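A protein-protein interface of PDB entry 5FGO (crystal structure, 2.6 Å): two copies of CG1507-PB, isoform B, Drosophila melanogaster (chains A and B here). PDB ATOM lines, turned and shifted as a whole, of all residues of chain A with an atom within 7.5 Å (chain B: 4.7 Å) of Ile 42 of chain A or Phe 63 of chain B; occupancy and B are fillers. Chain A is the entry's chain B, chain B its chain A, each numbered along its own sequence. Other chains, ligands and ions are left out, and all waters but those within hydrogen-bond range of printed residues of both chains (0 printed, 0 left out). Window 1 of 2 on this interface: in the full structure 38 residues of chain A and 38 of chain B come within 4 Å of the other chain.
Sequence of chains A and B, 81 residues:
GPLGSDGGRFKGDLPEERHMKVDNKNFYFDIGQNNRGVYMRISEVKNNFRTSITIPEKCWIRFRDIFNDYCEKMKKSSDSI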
ATOM      1  N   MET A  20      -9.628  -1.050 -29.276  1.00  0.00           N
ATOM      2  CA  MET A  20      -9.816  -1.664 -30.591  1.00  0.00           C
ATOM      3  C   MET A  20     -10.015  -0.576 -31.622  1.00  0.00           C
ATOM      4  O   MET A  20     -10.529   0.477 -31.299  1.00  0.00           O
ATOM      5  CB  MET A  20     -11.015  -2.623 -30.598  1.00  0.00           C
ATOM      6  CG  MET A  20     -11.255  -3.324 -31.944  1.00  0.00           C
ATOM      7  SD  MET A  20     -12.742  -4.585 -31.904  1.00  0.00           S
ATOM      8  CE  MET A  20     -13.156  -4.194 -30.054  1.00  0.00           C
ATOM      9  N   ASN A  26     -12.847   4.438 -32.633  1.00  0.00           N
ATOM     10  CA  ASN A  26     -12.126   3.662 -31.648  1.00  0.00           C
ATOM     11  C   ASN A  26     -13.003   3.174 -30.505  1.00  0.00           C
ATOM     12  O   ASN A  26     -13.830   3.928 -29.978  1.00  0.00           O
ATOM     13  CB  ASN A  26     -11.002   4.508 -31.055  1.00  0.00           C
ATOM     14  CG  ASN A  26      -9.945   4.846 -32.058  1.00  0.00           C
ATOM     15  OD1 ASN A  26      -8.962   4.143 -32.203  1.00  0.00           O
ATOM     16  ND2 ASN A  26     -10.139   5.941 -32.756  1.00  0.00           N
ATOM     17  N   PHE A  27     -12.768   1.939 -30.073  1.00  0.00           N
ATOM     18  CA  PHE A  27     -13.432   1.394 -28.892  1.00  0.00           C
ATOM     19  C   PHE A  27     -12.508   1.236 -27.682  1.00  0.00           C
ATOM     20  O   PHE A  27     -11.384   0.749 -27.790  1.00  0.00           O
ATOM     21  CB  PHE A  27     -14.062   0.057 -29.237  1.00  0.00           C
ATOM     22  CG  PHE A  27     -15.337   0.158 -30.043  1.00  0.00           C
ATOM     23  CD1 PHE A  27     -16.557   0.369 -29.408  1.00  0.00           C
ATOM     24  CD2 PHE A  27     -15.333   0.017 -31.417  1.00  0.00           C
ATOM     25  CE1 PHE A  27     -17.731   0.422 -30.118  1.00  0.00           C
ATOM     26  CE2 PHE A  27     -16.532   0.084 -32.140  1.00  0.00           C
ATOM     27  CZ  PHE A  27     -17.721   0.280 -31.487  1.00  0.00           C
ATOM     28  N   TYR A  28     -12.975   1.675 -26.524  1.00  0.00           N
ATOM     29  CA  TYR A  28     -12.204   1.496 -25.303  1.00  0.00           C
ATOM     30  C   TYR A  28     -12.921   0.665 -24.284  1.00  0.00           C
ATOM     31  O   TYR A  28     -14.127   0.763 -24.160  1.00  0.00           O
ATOM     32  CB  TYR A  28     -11.835   2.846 -24.713  1.00  0.00           C
ATOM     33  CG  TYR A  28     -10.939   3.627 -25.638  1.00  0.00           C
ATOM     34  CD1 TYR A  28      -9.571   3.385 -25.662  1.00  0.00           C
ATOM     35  CD2 TYR A  28     -11.453   4.564 -26.519  1.00  0.00           C
ATOM     36  CE1 TYR A  28      -8.748   4.060 -26.517  1.00  0.00           C
ATOM     37  CE2 TYR A  28     -10.640   5.254 -27.369  1.00  0.00           C
ATOM     38  CZ  TYR A  28      -9.287   5.002 -27.367  1.00  0.00           C
ATOM     39  OH  TYR A  28      -8.452   5.679 -28.217  1.00  0.00           O
ATOM     40  N   PHE A  29     -12.164  -0.147 -23.556  1.00  0.00           N
ATOM     41  CA  PHE A  29     -12.686  -1.002 -22.496  1.00  0.00           C
ATOM     42  C   PHE A  29     -11.975  -0.675 -21.211  1.00  0.00           C
ATOM     43  O   PHE A  29     -10.755  -0.807 -21.140  1.00  0.00           O
ATOM     44  CB  PHE A  29     -12.457  -2.473 -22.825  1.00  0.00           C
ATOM     45  CG  PHE A  29     -12.979  -2.901 -24.179  1.00  0.00           C
ATOM     46  CD1 PHE A  29     -12.351  -2.474 -25.354  1.00  0.00           C
ATOM     47  CD2 PHE A  29     -14.049  -3.785 -24.274  1.00  0.00           C
ATOM     48  CE1 PHE A  29     -12.812  -2.870 -26.582  1.00  0.00           C
ATOM     49  CE2 PHE A  29     -14.512  -4.209 -25.499  1.00  0.00           C
ATOM     50  CZ  PHE A  29     -13.901  -3.748 -26.659  1.00  0.00           C
ATOM     51  N   ASP A  30     -12.685  -0.157 -20.227  1.00  0.00           N
ATOM     52  CA  ASP A  30     -12.078   0.030 -18.921  1.00  0.00           C
ATOM     53  C   ASP A  30     -12.919  -0.517 -17.771  1.00  0.00           C
ATOM     54  O   ASP A  30     -14.132  -0.600 -17.858  1.00  0.00           O
ATOM     55  CB  ASP A  30     -11.699   1.493 -18.696  1.00  0.00           C
ATOM     56  CG  ASP A  30     -12.769   2.432 -19.083  1.00  0.00           C
ATOM     57  OD1 ASP A  30     -12.879   2.689 -20.304  1.00  0.00           O
ATOM     58  OD2 ASP A  30     -13.481   2.929 -18.184  1.00  0.00           O
ATOM     59  N   TYR A  39     -17.744  -3.003 -12.840  1.00  0.00           N
ATOM     60  CA  TYR A  39     -18.392  -2.870 -14.132  1.00  0.00           C
ATOM     61  C   TYR A  39     -17.379  -2.687 -15.271  1.00  0.00           C
ATOM     62  O   TYR A  39     -16.211  -2.334 -15.039  1.00  0.00           O
ATOM     63  CB  TYR A  39     -19.371  -1.693 -14.103  1.00  0.00           C
ATOM     64  CG  TYR A  39     -18.710  -0.354 -13.817  1.00  0.00           C
ATOM     65  CD1 TYR A  39     -18.095   0.378 -14.827  1.00  0.00           C
ATOM     66  CD2 TYR A  39     -18.665   0.155 -12.524  1.00  0.00           C
ATOM     67  CE1 TYR A  39     -17.480   1.598 -14.552  1.00  0.00           C
ATOM     68  CE2 TYR A  39     -18.054   1.357 -12.241  1.00  0.00           C
ATOM     69  CZ  TYR A  39     -17.470   2.081 -13.253  1.00  0.00           C
ATOM     70  OH  TYR A  39     -16.868   3.281 -12.953  1.00  0.00           O
ATOM     71  N   MET A  40     -17.853  -2.928 -16.495  1.00  0.00           N
ATOM     72  CA  MET A  40     -17.089  -2.686 -17.708  1.00  0.00           C
ATOM     73  C   MET A  40     -17.734  -1.558 -18.527  1.00  0.00           C
ATOM     74  O   MET A  40     -18.893  -1.649 -18.923  1.00  0.00           O
ATOM     75  CB  MET A  40     -16.996  -3.955 -18.562  1.00  0.00           C
ATOM     76  CG  MET A  40     -16.049  -3.816 -19.741  1.00  0.00           C
ATOM     77  SD  MET A  40     -16.243  -5.178 -21.096  1.00  0.00           S
ATOM     78  CE  MET A  40     -15.915  -6.669 -19.924  1.00  0.00           C
ATOM     79  N   ARG A  41     -16.979  -0.494 -18.773  1.00  0.00           N
ATOM     80  CA  ARG A  41     -17.435   0.567 -19.640  1.00  0.00           C
ATOM     81  C   ARG A  41     -16.877   0.337 -21.030  1.00  0.00           C
ATOM     82  O   ARG A  41     -15.674   0.195 -21.196  1.00  0.00           O
ATOM     83  CB  ARG A  41     -17.001   1.929 -19.111  1.00  0.00           C
ATOM     84  CG  ARG A  41     -17.513   3.110 -19.931  1.00  0.00           C
ATOM     85  CD  ARG A  41     -17.041   4.423 -19.334  1.00  0.00           C
ATOM     86  NE  ARG A  41     -15.593   4.570 -19.527  1.00  0.00           N
ATOM     87  CZ  ARG A  41     -14.842   5.560 -19.036  1.00  0.00           C
ATOM     88  NH1 ARG A  41     -15.396   6.543 -18.328  1.00  0.00           N
ATOM     89  NH2 ARG A  41     -13.527   5.572 -19.265  1.00  0.00           N
ATOM     90  N   ILE A  42     -17.743   0.276 -22.028  1.00  0.00           N
ATOM     91  CA  ILE A  42     -17.266   0.171 -23.390  1.00  0.00           C
ATOM     92  C   ILE A  42     -17.581   1.492 -24.095  1.00  0.00           C
ATOM     93  O   ILE A  42     -18.735   1.848 -24.293  1.00  0.00           O
ATOM     94  CB  ILE A  42     -17.892  -1.014 -24.124  1.00  0.00           C
ATOM     95  CG1 ILE A  42     -17.818  -2.256 -23.252  1.00  0.00           C
ATOM     96  CG2 ILE A  42     -17.223  -1.233 -25.484  1.00  0.00           C
ATOM     97  CD1 ILE A  42     -18.433  -3.470 -23.879  1.00  0.00           C
ATOM     98  N   SER A  43     -16.548   2.230 -24.471  1.00  0.00           N
ATOM     99  CA  SER A  43     -16.772   3.521 -25.095  1.00  0.00           C
ATOM    100  C   SER A  43     -16.608   3.496 -26.594  1.00  0.00           C
ATOM    101  O   SER A  43     -15.729   2.827 -27.116  1.00  0.00           O
ATOM    102  CB  SER A  43     -15.828   4.546 -24.494  1.00  0.00           C
ATOM    103  OG  SER A  43     -15.920   4.509 -23.082  1.00  0.00           O
ATOM    104  N   GLU A  44     -17.458   4.247 -27.279  1.00  0.00           N
ATOM    105  CA  GLU A  44     -17.299   4.437 -28.695  1.00  0.00           C
ATOM    106  C   GLU A  44     -16.899   5.903 -28.843  1.00  0.00           C
ATOM    107  O   GLU A  44     -17.613   6.826 -28.421  1.00  0.00           O
ATOM    108  CB  GLU A  44     -18.591   4.135 -29.437  1.00  0.00           C
ATOM    109  CG  GLU A  44     -18.476   4.082 -30.950  1.00  0.00           C
ATOM    110  CD  GLU A  44     -19.812   3.825 -31.620  1.00  0.00           C
ATOM    111  OE1 GLU A  44     -20.785   3.471 -30.946  1.00  0.00           O
ATOM    112  OE2 GLU A  44     -19.898   3.958 -32.845  1.00  0.00           O
ATOM    113  N   VAL A  45     -15.721   6.097 -29.410  1.00  0.00           N
ATOM    114  CA  VAL A  45     -15.121   7.407 -29.561  1.00  0.00           C
ATOM    115  C   VAL A  45     -14.732   7.653 -30.994  1.00  0.00           C
ATOM    116  O   VAL A  45     -14.012   6.843 -31.585  1.00  0.00           O
ATOM    117  CB  VAL A  45     -13.877   7.563 -28.689  1.00  0.00           C
ATOM    118  CG1 VAL A  45     -13.258   8.935 -28.921  1.00  0.00           C
ATOM    119  CG2 VAL A  45     -14.228   7.352 -27.237  1.00  0.00           C
ATOM    120  N   THR A  51     -19.736   8.146 -26.798  1.00  0.00           N
ATOM    121  CA  THR A  51     -20.832   7.512 -26.055  1.00  0.00           C
ATOM    122  C   THR A  51     -20.318   6.203 -25.471  1.00  0.00           C
ATOM    123  O   THR A  51     -19.297   5.695 -25.911  1.00  0.00           O
ATOM    124  CB  THR A  51     -22.072   7.277 -26.936  1.00  0.00           C
ATOM    125  OG1 THR A  51     -23.218   6.986 -26.109  1.00  0.00           O
ATOM    126  CG2 THR A  51     -21.823   6.141 -27.889  1.00  0.00           C
ATOM    127  N   SER A  52     -20.979   5.689 -24.444  1.00  0.00           N
ATOM    128  CA  SER A  52     -20.529   4.459 -23.794  1.00  0.00           C
ATOM    129  C   SER A  52     -21.686   3.649 -23.229  1.00  0.00           C
ATOM    130  O   SER A  52     -22.808   4.129 -23.147  1.00  0.00           O
ATOM    131  CB  SER A  52     -19.533   4.756 -22.682  1.00  0.00           C
ATOM    132  OG  SER A  52     -20.162   5.368 -21.573  1.00  0.00           O
ATOM    133  N   ILE A  53     -21.415   2.389 -22.926  1.00  0.00           N
ATOM    134  CA  ILE A  53     -22.311   1.582 -22.113  1.00  0.00           C
ATOM    135  C   ILE A  53     -21.592   1.007 -20.896  1.00  0.00           C
ATOM    136  O   ILE A  53     -20.376   0.850 -20.887  1.00  0.00           O
ATOM    137  CB  ILE A  53     -22.915   0.423 -22.884  1.00  0.00           C
ATOM    138  CG1 ILE A  53     -21.778  -0.448 -23.444  1.00  0.00           C
ATOM    139  CG2 ILE A  53     -23.847   0.959 -23.955  1.00  0.00           C
ATOM    140  CD1 ILE A  53     -22.224  -1.745 -24.031  1.00  0.00           C
ATOM    141  N   THR A  54     -22.365   0.694 -19.871  1.00  0.00           N
ATOM    142  CA  THR A  54     -21.825   0.207 -18.627  1.00  0.00           C
ATOM    143  C   THR A  54     -22.479  -1.122 -18.240  1.00  0.00           C
ATOM    144  O   THR A  54     -23.694  -1.223 -18.064  1.00  0.00           O
ATOM    145  CB  THR A  54     -21.990   1.257 -17.527  1.00  0.00           C
ATOM    146  OG1 THR A  54     -20.982   2.246 -17.716  1.00  0.00           O
ATOM    147  CG2 THR A  54     -21.749   0.664 -16.170  1.00  0.00           C
ATOM    148  N   ILE A  55     -21.635  -2.138 -18.107  1.00  0.00           N
ATOM    149  CA  ILE A  55     -22.072  -3.500 -17.882  1.00  0.00           C
ATOM    150  C   ILE A  55     -21.566  -3.930 -16.541  1.00  0.00           C
ATOM    151  O   ILE A  55     -20.359  -3.936 -16.327  1.00  0.00           O
ATOM    152  CB  ILE A  55     -21.530  -4.462 -18.935  1.00  0.00           C
ATOM    153  CG1 ILE A  55     -21.795  -3.932 -20.334  1.00  0.00           C
ATOM    154  CG2 ILE A  55     -22.138  -5.825 -18.774  1.00  0.00           C
ATOM    155  CD1 ILE A  55     -20.967  -4.591 -21.388  1.00  0.00           C
ATOM    156  N   PHE A  63     -23.421 -11.789 -21.383  1.00  0.00           N
ATOM    157  CA  PHE A  63     -22.933 -11.008 -22.504  1.00  0.00           C
ATOM    158  C   PHE A  63     -22.028 -11.779 -23.465  1.00  0.00           C
ATOM    159  O   PHE A  63     -22.229 -11.799 -24.681  1.00  0.00           O
ATOM    160  CB  PHE A  63     -22.163  -9.834 -21.949  1.00  0.00           C
ATOM    161  CG  PHE A  63     -22.666  -8.523 -22.388  1.00  0.00           C
ATOM    162  CD1 PHE A  63     -23.697  -7.905 -21.702  1.00  0.00           C
ATOM    163  CD2 PHE A  63     -22.098  -7.878 -23.467  1.00  0.00           C
ATOM    164  CE1 PHE A  63     -24.163  -6.665 -22.092  1.00  0.00           C
ATOM    165  CE2 PHE A  63     -22.552  -6.638 -23.862  1.00  0.00           C
ATOM    166  CZ  PHE A  63     -23.584  -6.037 -23.181  1.00  0.00           C
ATOM    167  N   PHE A  67     -22.482 -12.979 -27.447  1.00  0.00           N
ATOM    168  CA  PHE A  67     -21.487 -12.755 -28.475  1.00  0.00           C
ATOM    169  C   PHE A  67     -21.019 -13.985 -29.233  1.00  0.00           C
ATOM    170  O   PHE A  67     -20.874 -13.914 -30.465  1.00  0.00           O
ATOM    171  CB  PHE A  67     -20.306 -11.998 -27.906  1.00  0.00           C
ATOM    172  CG  PHE A  67     -20.324 -10.585 -28.320  1.00  0.00           C
ATOM    173  CD1 PHE A  67     -21.179  -9.689 -27.698  1.00  0.00           C
ATOM    174  CD2 PHE A  67     -19.603 -10.179 -29.433  1.00  0.00           C
ATOM    175  CE1 PHE A  67     -21.245  -8.379 -28.113  1.00  0.00           C
ATOM    176  CE2 PHE A  67     -19.654  -8.877 -29.866  1.00  0.00           C
ATOM    177  CZ  PHE A  67     -20.473  -7.971 -29.198  1.00  0.00           C
ATOM    178  N   CYS A  71     -21.195 -14.607 -33.135  1.00  0.00           N
ATOM    179  CA  CYS A  71     -19.983 -14.984 -33.885  1.00  0.00           C
ATOM    180  C   CYS A  71     -20.016 -16.341 -34.600  1.00  0.00           C
ATOM    181  O   CYS A  71     -19.416 -16.494 -35.675  1.00  0.00           O
ATOM    182  CB  CYS A  71     -18.775 -15.007 -32.941  1.00  0.00           C
ATOM    183  SG  CYS A  71     -18.241 -13.421 -32.300  1.00  0.00           S
ATOM    184  N   ILE B  53     -23.869   1.629 -28.545  1.00  0.00           N
ATOM    185  CA  ILE B  53     -22.651   1.564 -29.336  1.00  0.00           C
ATOM    186  C   ILE B  53     -22.967   0.668 -30.497  1.00  0.00           C
ATOM    187  O   ILE B  53     -23.845  -0.189 -30.397  1.00  0.00           O
ATOM    188  CB  ILE B  53     -21.487   0.987 -28.557  1.00  0.00           C
ATOM    189  CG1 ILE B  53     -21.815  -0.445 -28.086  1.00  0.00           C
ATOM    190  CG2 ILE B  53     -21.123   1.895 -27.403  1.00  0.00           C
ATOM    191  CD1 ILE B  53     -20.652  -1.223 -27.479  1.00  0.00           C
ATOM    192  N   ILE B  55     -21.372  -1.819 -33.521  1.00  0.00           N
ATOM    193  CA  ILE B  55     -20.190  -2.561 -33.899  1.00  0.00           C
ATOM    194  C   ILE B  55     -20.328  -3.223 -35.248  1.00  0.00           C
ATOM    195  O   ILE B  55     -21.190  -4.063 -35.463  1.00  0.00           O
ATOM    196  CB  ILE B  55     -19.901  -3.590 -32.853  1.00  0.00           C
ATOM    197  CG1 ILE B  55     -19.775  -2.886 -31.504  1.00  0.00           C
ATOM    198  CG2 ILE B  55     -18.638  -4.305 -33.174  1.00  0.00           C
ATOM    199  CD1 ILE B  55     -19.928  -3.791 -30.340  1.00  0.00           C
ATOM    200  N   CYS B  59     -15.500  -6.745 -37.073  1.00  0.00           N
ATOM    201  CA  CYS B  59     -14.749  -6.756 -35.844  1.00  0.00           C
ATOM    202  C   CYS B  59     -15.456  -7.471 -34.719  1.00  0.00           C
ATOM    203  O   CYS B  59     -15.031  -7.371 -33.555  1.00  0.00           O
ATOM    204  CB  CYS B  59     -14.436  -5.330 -35.443  1.00  0.00           C
ATOM    205  SG  CYS B  59     -15.897  -4.429 -34.891  1.00  0.00           S
ATOM    206  N   TRP B  60     -16.501  -8.233 -35.056  1.00  0.00           N
ATOM    207  CA  TRP B  60     -17.207  -9.006 -34.031  1.00  0.00           C
ATOM    208  C   TRP B  60     -16.281  -9.992 -33.330  1.00  0.00           C
ATOM    209  O   TRP B  60     -16.359 -10.151 -32.113  1.00  0.00           O
ATOM    210  CB  TRP B  60     -18.415  -9.754 -34.596  1.00  0.00           C
ATOM    211  CG  TRP B  60     -19.585  -8.882 -34.997  1.00  0.00           C
ATOM    212  CD1 TRP B  60     -19.649  -7.511 -34.978  1.00  0.00           C
ATOM    213  CD2 TRP B  60     -20.886  -9.335 -35.410  1.00  0.00           C
ATOM    214  NE1 TRP B  60     -20.891  -7.090 -35.396  1.00  0.00           N
ATOM    215  CE2 TRP B  60     -21.668  -8.188 -35.666  1.00  0.00           C
ATOM    216  CE3 TRP B  60     -21.458 -10.600 -35.613  1.00  0.00           C
ATOM    217  CZ2 TRP B  60     -22.992  -8.272 -36.116  1.00  0.00           C
ATOM    218  CZ3 TRP B  60     -22.772 -10.677 -36.055  1.00  0.00           C
ATOM    219  CH2 TRP B  60     -23.524  -9.525 -36.297  1.00  0.00           C
ATOM    220  N   ILE B  61     -15.410 -10.658 -34.082  1.00  0.00           N
ATOM    221  CA  ILE B  61     -14.511 -11.608 -33.446  1.00  0.00           C
ATOM    222  C   ILE B  61     -13.544 -10.951 -32.486  1.00  0.00           C
ATOM    223  O   ILE B  61     -13.451 -11.354 -31.324  1.00  0.00           O
ATOM    224  CB  ILE B  61     -13.716 -12.388 -34.466  1.00  0.00           C
ATOM    225  CG1 ILE B  61     -14.659 -13.324 -35.195  1.00  0.00           C
ATOM    226  CG2 ILE B  61     -12.652 -13.217 -33.789  1.00  0.00           C
ATOM    227  CD1 ILE B  61     -14.007 -13.970 -36.304  1.00  0.00           C
ATOM    228  N   ARG B  62     -12.839  -9.932 -32.961  1.00  0.00           N
ATOM    229  CA  ARG B  62     -11.906  -9.225 -32.098  1.00  0.00           C
ATOM    230  C   ARG B  62     -12.603  -8.681 -30.850  1.00  0.00           C
ATOM    231  O   ARG B  62     -12.064  -8.789 -29.748  1.00  0.00           O
ATOM    232  CB  ARG B  62     -11.200  -8.104 -32.871  1.00  0.00           C
ATOM    233  CG  ARG B  62     -10.182  -7.340 -32.058  1.00  0.00           C
ATOM    234  CD  ARG B  62      -9.123  -8.251 -31.439  1.00  0.00           C
ATOM    235  NE  ARG B  62      -8.138  -7.485 -30.674  1.00  0.00           N
ATOM    236  CZ  ARG B  62      -7.172  -8.003 -29.916  1.00  0.00           C
ATOM    237  NH1 ARG B  62      -7.016  -9.320 -29.786  1.00  0.00           N
ATOM    238  NH2 ARG B  62      -6.358  -7.190 -29.269  1.00  0.00           N
ATOM    239  N   PHE B  63     -13.799  -8.109 -31.035  1.00  0.00           N
ATOM    240  CA  PHE B  63     -14.636  -7.600 -29.926  1.00  0.00           C
ATOM    241  C   PHE B  63     -15.022  -8.732 -28.943  1.00  0.00           C
ATOM    242  O   PHE B  63     -15.008  -8.557 -27.715  1.00  0.00           O
ATOM    243  CB  PHE B  63     -15.876  -6.885 -30.471  1.00  0.00           C
ATOM    244  CG  PHE B  63     -16.653  -6.111 -29.424  1.00  0.00           C
ATOM    245  CD1 PHE B  63     -17.590  -6.734 -28.621  1.00  0.00           C
ATOM    246  CD2 PHE B  63     -16.449  -4.746 -29.251  1.00  0.00           C
ATOM    247  CE1 PHE B  63     -18.303  -6.018 -27.663  1.00  0.00           C
ATOM    248  CE2 PHE B  63     -17.163  -4.025 -28.292  1.00  0.00           C
ATOM    249  CZ  PHE B  63     -18.095  -4.664 -27.505  1.00  0.00           C
ATOM    250  N   ARG B  64     -15.415  -9.879 -29.488  1.00  0.00           N
ATOM    251  CA  ARG B  64     -15.671 -11.043 -28.656  1.00  0.00           C
ATOM    252  C   ARG B  64     -14.466 -11.482 -27.828  1.00  0.00           C
ATOM    253  O   ARG B  64     -14.591 -11.796 -26.640  1.00  0.00           O
ATOM    254  CB  ARG B  64     -16.109 -12.217 -29.519  1.00  0.00           C
ATOM    255  CG  ARG B  64     -16.725 -13.357 -28.740  1.00  0.00           C
ATOM    256  CD  ARG B  64     -16.098 -14.685 -29.170  1.00  0.00           C
ATOM    257  NE  ARG B  64     -14.846 -15.016 -28.481  1.00  0.00           N
ATOM    258  CZ  ARG B  64     -14.756 -15.845 -27.438  1.00  0.00           C
ATOM    259  NH1 ARG B  64     -15.843 -16.419 -26.931  1.00  0.00           N
ATOM    260  NH2 ARG B  64     -13.574 -16.103 -26.895  1.00  0.00           N
ATOM    261  N   ASP B  65     -13.294 -11.502 -28.449  1.00  0.00           N
ATOM    262  CA  ASP B  65     -12.118 -11.992 -27.742  1.00  0.00           C
ATOM    263  C   ASP B  65     -11.730 -11.050 -26.613  1.00  0.00           C
ATOM    264  O   ASP B  65     -11.374 -11.476 -25.506  1.00  0.00           O
ATOM    265  CB  ASP B  65     -10.948 -12.205 -28.694  1.00  0.00           C
ATOM    266  CG  ASP B  65     -11.223 -13.289 -29.691  1.00  0.00           C
ATOM    267  OD1 ASP B  65     -12.132 -14.099 -29.424  1.00  0.00           O
ATOM    268  OD2 ASP B  65     -10.515 -13.366 -30.715  1.00  0.00           O
ATOM    269  N   ILE B  66     -11.771  -9.766 -26.901  1.00  0.00           N
ATOM    270  CA  ILE B  66     -11.446  -8.806 -25.886  1.00  0.00           C
ATOM    271  C   ILE B  66     -12.396  -8.963 -24.708  1.00  0.00           C
ATOM    272  O   ILE B  66     -11.969  -8.964 -23.543  1.00  0.00           O
ATOM    273  CB  ILE B  66     -11.475  -7.395 -26.477  1.00  0.00           C
ATOM    274  CG1 ILE B  66     -10.229  -7.244 -27.370  1.00  0.00           C
ATOM    275  CG2 ILE B  66     -11.521  -6.365 -25.375  1.00  0.00           C
ATOM    276  CD1 ILE B  66     -10.195  -6.011 -28.266  1.00  0.00           C
ATOM    277  N   PHE B  67     -13.681  -9.127 -25.006  1.00  0.00           N
ATOM    278  CA  PHE B  67     -14.652  -9.272 -23.933  1.00  0.00           C
ATOM    279  C   PHE B  67     -14.368 -10.564 -23.191  1.00  0.00           C
ATOM    280  O   PHE B  67     -14.391 -10.605 -21.966  1.00  0.00           O
ATOM    281  CB  PHE B  67     -16.102  -9.254 -24.438  1.00  0.00           C
ATOM    282  CG  PHE B  67     -17.112  -9.109 -23.330  1.00  0.00           C
ATOM    283  CD1 PHE B  67     -17.463 -10.186 -22.535  1.00  0.00           C
ATOM    284  CD2 PHE B  67     -17.718  -7.885 -23.088  1.00  0.00           C
ATOM    285  CE1 PHE B  67     -18.372 -10.042 -21.499  1.00  0.00           C
ATOM    286  CE2 PHE B  67     -18.649  -7.736 -22.064  1.00  0.00           C
ATOM    287  CZ  PHE B  67     -18.970  -8.815 -21.265  1.00  0.00           C
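O of Cys 59 of chain B touches SD of Met 20 of chain A, at 3.97 Å.
Phe 29 of chain A touches Phe 63 of chain B (CZ to CE2, 3.7 Å).
Ile 66 of chain B touches Phe 29 of chain A (CG2 to CE2, 3.7 Å).
Met 40 of chain A touches Phe 67 of chain B (CE to CE2, 3.6 Å).
Ile 42 of chain A touches Phe 63 of chain B (CD1 to CZ, 3.8 Å).
OE1 of Glu 44 of chain A touches CA of Ile 53 of chain B (3.1 Å).
CD1 of Ile 53 of chain A touches CD1 of Ile 53 of chain B, at 3.8 Å.
CE2 of Phe 67 of chain B touches CD1 of Ile 55 of chain A, 3.96 Å away.
Phe 63 of chain A touches Phe 67 of chain B.
Phe 67 of chain A touches Phe 63 of chain B (CZ to CD1, 3.2 Å).
The backbone carbonyl oxygen (O) of Ile 55 of chain B sits at hydrogen-bond distance from the indole nitrogen (NE1) of Trp 60 of chain B (3.0 Å).
NE of Arg 64 of chain B lies within salt-bridge range of OD1 of Asp 65 of chain B.
N of Met 20 of chain A is in hydrogen-bond range of O of Phe 27 of chain A.
The backbone NH of Met 40 of chain A is in hydrogen-bond range of the backbone carbonyl oxygen of Ile 55 of chain A.
The backbone NH of Ile 42 of chain A sits at hydrogen-bond distance from the backbone carbonyl oxygen of Ile 53 of chain A (2.9 Å).
The backbone NH of Glu 44 of chain A sits at hydrogen-bond distance from the backbone carbonyl oxygen of Thr 51 of chain A (2.7 Å).
Phe 63 of chain B touches four residues of chain A.
Printed residues of chain A within 4 Å of Ile 55 of chain B: Phe 27 (3.8 Å).
Printed residues of chain A within 4 Å of Arg 62 of chain B: Met 20 (3.8 Å).
Printed residues of chain B within 4 Å of Phe 29 of chain A: Phe 63 (3.7 Å) and Ile 66 (3.7 Å).
Thr 51 of chain A touches none of the printed residues of chain B.
The nearest printed residue of chain B that does not touch Phe 27 of chain A is Ile 53 of chain B (4.1 Å).
Ile 53 of chain A touches its own counterpart, Ile 53 of chain B.
Ile 55 of chain A touches Phe 67 of chain B, but with the chains exchanged Phe 67 of chain A does not touch Ile 55 of chain B (4.4 Å).
Phe 63 of chain A touches Phe 67 of chain B, and with the chains exchanged Phe 67 of chain A touches Phe 63 of chain B.
Of the 18 pairs that touch across the chains among the printed residues, 3 have their exchanged pair printed and touching as well.
The side-chain sulfur (SG) of Cys 71 of chain A lies within hydrogen-bond range of the backbone carbonyl oxygen (O) of Trp 60 of chain B, 3.8 Å away.
The side-chain sulfur (SD) of Met 20 of chain A sits at hydrogen-bond distance from the backbone NH (N) of Phe 63 of chain B (3.8 Å).
Printed residues of chain B that touch a printed residue of chain A: Ile 53, Ile 55, Cys 59, Trp 60, Arg 62, Phe 63, Arg 64, Ile 66 and Phe 67.
Hydrophobic or aromatic side chains of chain B that line the printed part of chain A: Ile 53, Ile 55, Phe 63, Ile 66 and Phe 67.
Of the 21 printed residues of chain A, 11 touch a printed residue of chain B.
Hydrophobic or aromatic side chains of chain A within 4 Å of the printed part of chain B: Met 20, Phe 27, Phe 29, Met 40, Ile 42, Ile 53, Ile 55, Phe 63 and Phe 67.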
